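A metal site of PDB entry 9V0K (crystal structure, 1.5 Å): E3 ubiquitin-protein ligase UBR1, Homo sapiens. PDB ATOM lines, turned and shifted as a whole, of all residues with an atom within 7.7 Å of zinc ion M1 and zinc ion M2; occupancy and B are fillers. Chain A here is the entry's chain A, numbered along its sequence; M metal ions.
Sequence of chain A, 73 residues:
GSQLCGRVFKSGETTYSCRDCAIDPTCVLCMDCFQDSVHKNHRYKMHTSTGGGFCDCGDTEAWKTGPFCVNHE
N of Gln 3 lies within hydrogen-bond range of O of His 72. The backbone NH (N) of Cys 57 lies close to the side-chain sulfur (SG) of Cys 55. O of Cys 57 lies within hydrogen-bond range of N of Cys 5, 3.0 Å away. SG of Cys 69 lies close to N of Asn 71. The backbone carbonyl oxygen (O) of Arg 7 lies within hydrogen-bond range of the backbone NH (N) of Cys 55 (2.9 Å). The side-chain sulfur of Cys 5 lies close to the backbone NH of Arg 7, 3.5 Å away.
Within 4 Å of zinc ion M1: Cys 33, Cys 57, Cys 69 and His 72. The nearest printed residue that does not touch zinc ion M1 is Cys 5 (4.3 Å).
The nearest printed residue that does not touch zinc ion M2 is Cys 57 (4.1 Å).
Zinc ion M1 is bound by ND1 of His 72 (2.0 Å), SG of Cys 57 (2.3 Å), SG of Cys 69 (2.3 Å) and SG of Cys 33 (2.3 Å). Zinc ion M1 has four donor atoms within binding distance.
Zinc ion M2 is bound by the side-chain sulfur (SG) of Cys 55 (2.3 Å), the side-chain sulfur (SG) of Cys 30 (2.3 Å), the side-chain sulfur (SG) of Cys 5 (2.3 Å) and the side-chain sulfur (SG) of Cys 33 (2.4 Å).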
ATOM      1  N   GLN A   3      25.753 -30.398  18.582  1.00  0.00           N
ATOM      2  CA  GLN A   3      24.462 -30.095  18.004  1.00  0.00           C
ATOM      3  C   GLN A   3      24.068 -28.671  18.354  1.00  0.00           C
ATOM      4  O   GLN A   3      24.403 -28.168  19.420  1.00  0.00           O
ATOM      5  CB  GLN A   3      23.362 -30.999  18.569  1.00  0.00           C
ATOM      6  CG  GLN A   3      23.421 -32.451  18.183  1.00  0.00           C
ATOM      7  CD  GLN A   3      22.437 -33.281  18.982  1.00  0.00           C
ATOM      8  OE1 GLN A   3      22.336 -33.133  20.200  1.00  0.00           O
ATOM      9  NE2 GLN A   3      21.684 -34.131  18.289  1.00  0.00           N
ATOM     10  N   LEU A   4      23.261 -28.069  17.480  1.00  0.00           N
ATOM     11  CA  LEU A   4      22.582 -26.830  17.797  1.00  0.00           C
ATOM     12  C   LEU A   4      21.203 -27.135  18.370  1.00  0.00           C
ATOM     13  O   LEU A   4      20.488 -27.988  17.843  1.00  0.00           O
ATOM     14  CB  LEU A   4      22.392 -25.967  16.552  1.00  0.00           C
ATOM     15  CG  LEU A   4      23.602 -25.226  16.000  1.00  0.00           C
ATOM     16  CD1 LEU A   4      23.295 -24.867  14.560  1.00  0.00           C
ATOM     17  CD2 LEU A   4      23.935 -23.975  16.773  1.00  0.00           C
ATOM     18  N   CYS A   5      20.821 -26.396  19.405  1.00  0.00           N
ATOM     19  CA  CYS A   5      19.483 -26.588  19.975  1.00  0.00           C
ATOM     20  C   CYS A   5      18.404 -26.152  18.991  1.00  0.00           C
ATOM     21  O   CYS A   5      17.500 -26.919  18.665  1.00  0.00           O
ATOM     22  CB  CYS A   5      19.336 -25.810  21.287  1.00  0.00           C
ATOM     23  SG  CYS A   5      17.633 -25.839  21.867  1.00  0.00           S
ATOM     24  N   GLY A   6      18.452 -24.885  18.579  1.00  0.00           N
ATOM     25  CA  GLY A   6      17.534 -24.315  17.618  1.00  0.00           C
ATOM     26  C   GLY A   6      16.119 -24.050  18.090  1.00  0.00           C
ATOM     27  O   GLY A   6      15.289 -23.665  17.260  1.00  0.00           O
ATOM     28  N   ARG A   7      15.819 -24.219  19.380  1.00  0.00           N
ATOM     29  CA  ARG A   7      14.452 -24.063  19.856  1.00  0.00           C
ATOM     30  C   ARG A   7      13.963 -22.643  19.583  1.00  0.00           C
ATOM     31  O   ARG A   7      14.678 -21.673  19.833  1.00  0.00           O
ATOM     32  CB  ARG A   7      14.323 -24.389  21.356  1.00  0.00           C
ATOM     33  CG  ARG A   7      12.882 -24.238  21.861  1.00  0.00           C
ATOM     34  CD  ARG A   7      12.735 -24.368  23.384  1.00  0.00           C
ATOM     35  NE  ARG A   7      11.415 -23.917  23.790  1.00  0.00           N
ATOM     36  CZ  ARG A   7      10.296 -24.507  23.426  1.00  0.00           C
ATOM     37  NH1 ARG A   7      10.292 -25.682  22.815  1.00  0.00           N
ATOM     38  NH2 ARG A   7       9.128 -23.912  23.683  1.00  0.00           N
ATOM     39  N   VAL A   8      12.753 -22.534  19.046  1.00  0.00           N
ATOM     40  CA  VAL A   8      12.096 -21.245  18.837  1.00  0.00           C
ATOM     41  C   VAL A   8      11.118 -21.028  19.979  1.00  0.00           C
ATOM     42  O   VAL A   8      10.257 -21.876  20.259  1.00  0.00           O
ATOM     43  CB  VAL A   8      11.386 -21.195  17.473  1.00  0.00           C
ATOM     44  CG1 VAL A   8      10.574 -19.952  17.341  1.00  0.00           C
ATOM     45  CG2 VAL A   8      12.412 -21.239  16.320  1.00  0.00           C
ATOM     46  N   PHE A   9      11.249 -19.880  20.649  1.00  0.00           N
ATOM     47  CA  PHE A   9      10.504 -19.632  21.877  1.00  0.00           C
ATOM     48  C   PHE A   9       9.035 -19.368  21.581  1.00  0.00           C
ATOM     49  O   PHE A   9       8.668 -18.790  20.554  1.00  0.00           O
ATOM     50  CB  PHE A   9      11.101 -18.435  22.615  1.00  0.00           C
ATOM     51  CG  PHE A   9      12.567 -18.585  22.931  1.00  0.00           C
ATOM     52  CD1 PHE A   9      13.038 -19.638  23.696  1.00  0.00           C
ATOM     53  CD2 PHE A   9      13.469 -17.654  22.467  1.00  0.00           C
ATOM     54  CE1 PHE A   9      14.402 -19.765  23.966  1.00  0.00           C
ATOM     55  CE2 PHE A   9      14.808 -17.747  22.746  1.00  0.00           C
ATOM     56  CZ  PHE A   9      15.283 -18.826  23.497  1.00  0.00           C
ATOM     57  N   VAL A  28      21.005 -15.857  23.906  1.00  0.00           N
ATOM     58  CA  VAL A  28      20.006 -16.341  24.851  1.00  0.00           C
ATOM     59  C   VAL A  28      19.927 -17.857  24.799  1.00  0.00           C
ATOM     60  O   VAL A  28      20.319 -18.489  23.818  1.00  0.00           O
ATOM     61  CB  VAL A  28      18.639 -15.684  24.542  1.00  0.00           C
ATOM     62  CG1 VAL A  28      18.198 -15.987  23.103  1.00  0.00           C
ATOM     63  CG2 VAL A  28      17.604 -16.104  25.523  1.00  0.00           C
ATOM     64  N   LEU A  29      19.425 -18.457  25.889  1.00  0.00           N
ATOM     65  CA  LEU A  29      19.259 -19.888  25.989  1.00  0.00           C
ATOM     66  C   LEU A  29      17.833 -20.220  26.403  1.00  0.00           C
ATOM     67  O   LEU A  29      17.209 -19.456  27.133  1.00  0.00           O
ATOM     68  CB  LEU A  29      20.210 -20.520  27.037  1.00  0.00           C
ATOM     69  CG  LEU A  29      21.700 -20.319  26.751  1.00  0.00           C
ATOM     70  CD1 LEU A  29      22.493 -20.595  28.013  1.00  0.00           C
ATOM     71  CD2 LEU A  29      22.157 -21.267  25.646  1.00  0.00           C
ATOM     72  N   CYS A  30      17.344 -21.380  25.935  1.00  0.00           N
ATOM     73  CA  CYS A  30      16.112 -21.935  26.457  1.00  0.00           C
ATOM     74  C   CYS A  30      16.351 -22.502  27.850  1.00  0.00           C
ATOM     75  O   CYS A  30      17.482 -22.747  28.261  1.00  0.00           O
ATOM     76  CB  CYS A  30      15.547 -23.027  25.540  1.00  0.00           C
ATOM     77  SG  CYS A  30      16.440 -24.625  25.510  1.00  0.00           S
ATOM     78  N   MET A  31      15.263 -22.677  28.590  1.00  0.00           N
ATOM     79  CA  MET A  31      15.393 -23.180  29.946  1.00  0.00           C
ATOM     80  C   MET A  31      16.138 -24.517  29.999  1.00  0.00           C
ATOM     81  O   MET A  31      17.031 -24.692  30.840  1.00  0.00           O
ATOM     82  CB  MET A  31      14.023 -23.331  30.599  1.00  0.00           C
ATOM     83  CG  MET A  31      14.202 -23.463  32.091  1.00  0.00           C
ATOM     84  SD  MET A  31      14.124 -25.229  32.505  1.00  0.00           S
ATOM     85  CE  MET A  31      12.578 -25.783  31.730  1.00  0.00           C
ATOM     86  N   ASP A  32      15.738 -25.482  29.168  1.00  0.00           N
ATOM     87  CA  ASP A  32      16.357 -26.804  29.217  1.00  0.00           C
ATOM     88  C   ASP A  32      17.863 -26.717  29.065  1.00  0.00           C
ATOM     89  O   ASP A  32      18.617 -27.334  29.827  1.00  0.00           O
ATOM     90  CB  ASP A  32      15.773 -27.686  28.109  1.00  0.00           C
ATOM     91  CG  ASP A  32      14.434 -28.250  28.470  1.00  0.00           C
ATOM     92  OD1 ASP A  32      13.427 -27.560  28.256  1.00  0.00           O
ATOM     93  OD2 ASP A  32      14.412 -29.409  28.951  1.00  0.00           O
ATOM     94  N   CYS A  33      18.331 -25.945  28.080  1.00  0.00           N
ATOM     95  CA  CYS A  33      19.760 -25.811  27.859  1.00  0.00           C
ATOM     96  C   CYS A  33      20.421 -25.061  29.016  1.00  0.00           C
ATOM     97  O   CYS A  33      21.473 -25.469  29.499  1.00  0.00           O
ATOM     98  CB  CYS A  33      20.017 -25.097  26.521  1.00  0.00           C
ATOM     99  SG  CYS A  33      19.560 -26.138  25.071  1.00  0.00           S
ATOM    100  N   PHE A  34      19.803 -23.960  29.468  1.00  0.00           N
ATOM    101  CA  PHE A  34      20.369 -23.169  30.555  1.00  0.00           C
ATOM    102  C   PHE A  34      20.633 -24.030  31.785  1.00  0.00           C
ATOM    103  O   PHE A  34      21.743 -24.004  32.332  1.00  0.00           O
ATOM    104  CB  PHE A  34      19.437 -21.989  30.859  1.00  0.00           C
ATOM    105  CG  PHE A  34      19.755 -21.271  32.097  1.00  0.00           C
ATOM    106  CD1 PHE A  34      20.778 -20.338  32.134  1.00  0.00           C
ATOM    107  CD2 PHE A  34      19.000 -21.492  33.254  1.00  0.00           C
ATOM    108  CE1 PHE A  34      21.054 -19.646  33.308  1.00  0.00           C
ATOM    109  CE2 PHE A  34      19.276 -20.793  34.400  1.00  0.00           C
ATOM    110  CZ  PHE A  34      20.299 -19.878  34.433  1.00  0.00           C
ATOM    111  N   ASP A  36      21.115 -27.087  32.067  1.00  0.00           N
ATOM    112  CA  ASP A  36      22.094 -28.139  31.799  1.00  0.00           C
ATOM    113  C   ASP A  36      23.425 -27.544  31.329  1.00  0.00           C
ATOM    114  O   ASP A  36      24.197 -28.212  30.636  1.00  0.00           O
ATOM    115  CB  ASP A  36      21.550 -29.122  30.769  1.00  0.00           C
ATOM    116  CG  ASP A  36      20.896 -30.356  31.402  1.00  0.00           C
ATOM    117  OD1 ASP A  36      21.096 -30.617  32.604  1.00  0.00           O
ATOM    118  OD2 ASP A  36      20.165 -31.062  30.676  1.00  0.00           O
ATOM    119  N   SER A  37      23.698 -26.302  31.708  1.00  0.00           N
ATOM    120  CA  SER A  37      24.871 -25.562  31.236  1.00  0.00           C
ATOM    121  C   SER A  37      25.576 -24.890  32.397  1.00  0.00           C
ATOM    122  O   SER A  37      25.053 -24.753  33.504  1.00  0.00           O
ATOM    123  CB  SER A  37      24.480 -24.486  30.186  1.00  0.00           C
ATOM    124  OG  SER A  37      23.958 -23.317  30.849  1.00  0.00           O
ATOM    125  N   PHE A  54      15.174 -17.438  19.246  1.00  0.00           N
ATOM    126  CA  PHE A  54      15.641 -18.823  19.317  1.00  0.00           C
ATOM    127  C   PHE A  54      16.825 -18.997  20.267  1.00  0.00           C
ATOM    128  O   PHE A  54      17.604 -18.075  20.520  1.00  0.00           O
ATOM    129  CB  PHE A  54      16.011 -19.332  17.907  1.00  0.00           C
ATOM    130  CG  PHE A  54      17.004 -18.440  17.195  1.00  0.00           C
ATOM    131  CD1 PHE A  54      16.566 -17.379  16.446  1.00  0.00           C
ATOM    132  CD2 PHE A  54      18.362 -18.687  17.271  1.00  0.00           C
ATOM    133  CE1 PHE A  54      17.461 -16.572  15.802  1.00  0.00           C
ATOM    134  CE2 PHE A  54      19.261 -17.873  16.620  1.00  0.00           C
ATOM    135  CZ  PHE A  54      18.811 -16.804  15.910  1.00  0.00           C
ATOM    136  N   CYS A  55      16.957 -20.220  20.761  1.00  0.00           N
ATOM    137  CA  CYS A  55      18.049 -20.598  21.650  1.00  0.00           C
ATOM    138  C   CYS A  55      19.354 -20.652  20.885  1.00  0.00           C
ATOM    139  O   CYS A  55      19.398 -21.205  19.786  1.00  0.00           O
ATOM    140  CB  CYS A  55      17.744 -21.959  22.252  1.00  0.00           C
ATOM    141  SG  CYS A  55      19.033 -22.640  23.310  1.00  0.00           S
ATOM    142  N   ASP A  56      20.422 -20.059  21.446  1.00  0.00           N
ATOM    143  CA  ASP A  56      21.761 -20.056  20.869  1.00  0.00           C
ATOM    144  C   ASP A  56      22.679 -21.173  21.399  1.00  0.00           C
ATOM    145  O   ASP A  56      23.890 -21.161  21.129  1.00  0.00           O
ATOM    146  CB  ASP A  56      22.407 -18.694  21.122  1.00  0.00           C
ATOM    147  CG  ASP A  56      21.656 -17.548  20.431  1.00  0.00           C
ATOM    148  OD1 ASP A  56      21.398 -17.660  19.209  1.00  0.00           O
ATOM    149  OD2 ASP A  56      21.295 -16.573  21.106  1.00  0.00           O
ATOM    150  N   CYS A  57      22.150 -22.144  22.121  1.00  0.00           N
ATOM    151  CA  CYS A  57      22.973 -23.264  22.542  1.00  0.00           C
ATOM    152  C   CYS A  57      23.529 -24.013  21.337  1.00  0.00           C
ATOM    153  O   CYS A  57      22.785 -24.381  20.428  1.00  0.00           O
ATOM    154  CB  CYS A  57      22.164 -24.212  23.408  1.00  0.00           C
ATOM    155  SG  CYS A  57      23.173 -25.596  23.985  1.00  0.00           S
ATOM    156  N   GLY A  58      24.833 -24.292  21.370  1.00  0.00           N
ATOM    157  CA  GLY A  58      25.505 -24.934  20.262  1.00  0.00           C
ATOM    158  C   GLY A  58      26.154 -23.994  19.286  1.00  0.00           C
ATOM    159  O   GLY A  58      26.916 -24.444  18.418  1.00  0.00           O
ATOM    160  N   PRO A  67      29.648 -22.958  25.201  1.00  0.00           N
ATOM    161  CA  PRO A  67      28.667 -22.814  24.113  1.00  0.00           C
ATOM    162  C   PRO A  67      27.674 -23.958  24.042  1.00  0.00           C
ATOM    163  O   PRO A  67      26.627 -23.790  23.417  1.00  0.00           O
ATOM    164  CB  PRO A  67      29.542 -22.750  22.862  1.00  0.00           C
ATOM    165  CG  PRO A  67      30.769 -23.518  23.247  1.00  0.00           C
ATOM    166  CD  PRO A  67      31.010 -23.166  24.691  1.00  0.00           C
ATOM    167  N   PHE A  68      27.947 -25.115  24.652  1.00  0.00           N
ATOM    168  CA  PHE A  68      27.044 -26.245  24.613  1.00  0.00           C
ATOM    169  C   PHE A  68      26.591 -26.603  26.013  1.00  0.00           C
ATOM    170  O   PHE A  68      27.413 -26.672  26.937  1.00  0.00           O
ATOM    171  CB  PHE A  68      27.696 -27.501  23.988  1.00  0.00           C
ATOM    172  CG  PHE A  68      28.167 -27.326  22.582  1.00  0.00           C
ATOM    173  CD1 PHE A  68      27.337 -27.623  21.523  1.00  0.00           C
ATOM    174  CD2 PHE A  68      29.444 -26.892  22.329  1.00  0.00           C
ATOM    175  CE1 PHE A  68      27.775 -27.466  20.230  1.00  0.00           C
ATOM    176  CE2 PHE A  68      29.891 -26.739  21.021  1.00  0.00           C
ATOM    177  CZ  PHE A  68      29.045 -27.010  19.982  1.00  0.00           C
ATOM    178  N   CYS A  69      25.307 -26.897  26.153  1.00  0.00           N
ATOM    179  CA  CYS A  69      24.825 -27.598  27.343  1.00  0.00           C
ATOM    180  C   CYS A  69      25.167 -29.085  27.246  1.00  0.00           C
ATOM    181  O   CYS A  69      25.678 -29.578  26.245  1.00  0.00           O
ATOM    182  CB  CYS A  69      23.321 -27.399  27.488  1.00  0.00           C
ATOM    183  SG  CYS A  69      22.340 -28.425  26.385  1.00  0.00           S
ATOM    184  N   VAL A  70      24.896 -29.827  28.324  1.00  0.00           N
ATOM    185  CA  VAL A  70      25.375 -31.218  28.343  1.00  0.00           C
ATOM    186  C   VAL A  70      24.543 -32.111  27.429  1.00  0.00           C
ATOM    187  O   VAL A  70      24.949 -33.256  27.157  1.00  0.00           O
ATOM    188  CB  VAL A  70      25.439 -31.779  29.774  1.00  0.00           C
ATOM    189  CG1 VAL A  70      26.465 -31.011  30.600  1.00  0.00           C
ATOM    190  CG2 VAL A  70      24.091 -31.779  30.439  1.00  0.00           C
ATOM    191  N   ASN A  71      23.426 -31.631  26.920  1.00  0.00           N
ATOM    192  CA  ASN A  71      22.600 -32.392  26.000  1.00  0.00           C
ATOM    193  C   ASN A  71      22.997 -32.189  24.558  1.00  0.00           C
ATOM    194  O   ASN A  71      22.774 -33.079  23.723  1.00  0.00           O
ATOM    195  CB  ASN A  71      21.135 -32.013  26.209  1.00  0.00           C
ATOM    196  CG  ASN A  71      20.701 -32.231  27.640  1.00  0.00           C
ATOM    197  OD1 ASN A  71      20.925 -33.290  28.216  1.00  0.00           O
ATOM    198  ND2 ASN A  71      20.132 -31.202  28.249  1.00  0.00           N
ATOM    199  N   HIS A  72      23.616 -31.067  24.255  1.00  0.00           N
ATOM    200  CA  HIS A  72      24.000 -30.727  22.888  1.00  0.00           C
ATOM    201  C   HIS A  72      25.492 -30.791  22.621  1.00  0.00           C
ATOM    202  O   HIS A  72      25.893 -30.769  21.449  1.00  0.00           O
ATOM    203  CB  HIS A  72      23.445 -29.337  22.564  1.00  0.00           C
ATOM    204  CG  HIS A  72      21.971 -29.330  22.434  1.00  0.00           C
ATOM    205  ND1 HIS A  72      21.155 -28.532  23.208  1.00  0.00           N
ATOM    206  CD2 HIS A  72      21.150 -30.042  21.634  1.00  0.00           C
ATOM    207  CE1 HIS A  72      19.894 -28.756  22.885  1.00  0.00           C
ATOM    208  NE2 HIS A  72      19.861 -29.680  21.932  1.00  0.00           N
ATOM    209  N   GLU A  73      26.317 -30.935  23.666  1.00  0.00           N
ATOM    210  CA  GLU A  73      27.721 -31.291  23.514  1.00  0.00           C
ATOM    211  C   GLU A  73      27.897 -32.550  22.643  1.00  0.00           C
ATOM    212  O   GLU A  73      28.721 -32.512  21.713  1.00  0.00           O
ATOM    213  CB  GLU A  73      28.367 -31.537  24.885  1.00  0.00           C
ATOM    214  CG  GLU A  73      29.881 -31.332  24.941  1.00  0.00           C
ATOM    215  CD  GLU A  73      30.312 -29.891  24.836  1.00  0.00           C
ATOM    216  OE1 GLU A  73      30.890 -29.510  23.790  1.00  0.00           O
ATOM    217  OE2 GLU A  73      30.053 -29.119  25.791  1.00  0.00           O
HETATM  218 ZN    ZN M   1      21.624 -27.151  24.620  1.00  0.00          ZN
HETATM  219 ZN    ZN M   2      18.099 -24.686  23.858  1.00  0.00          ZN
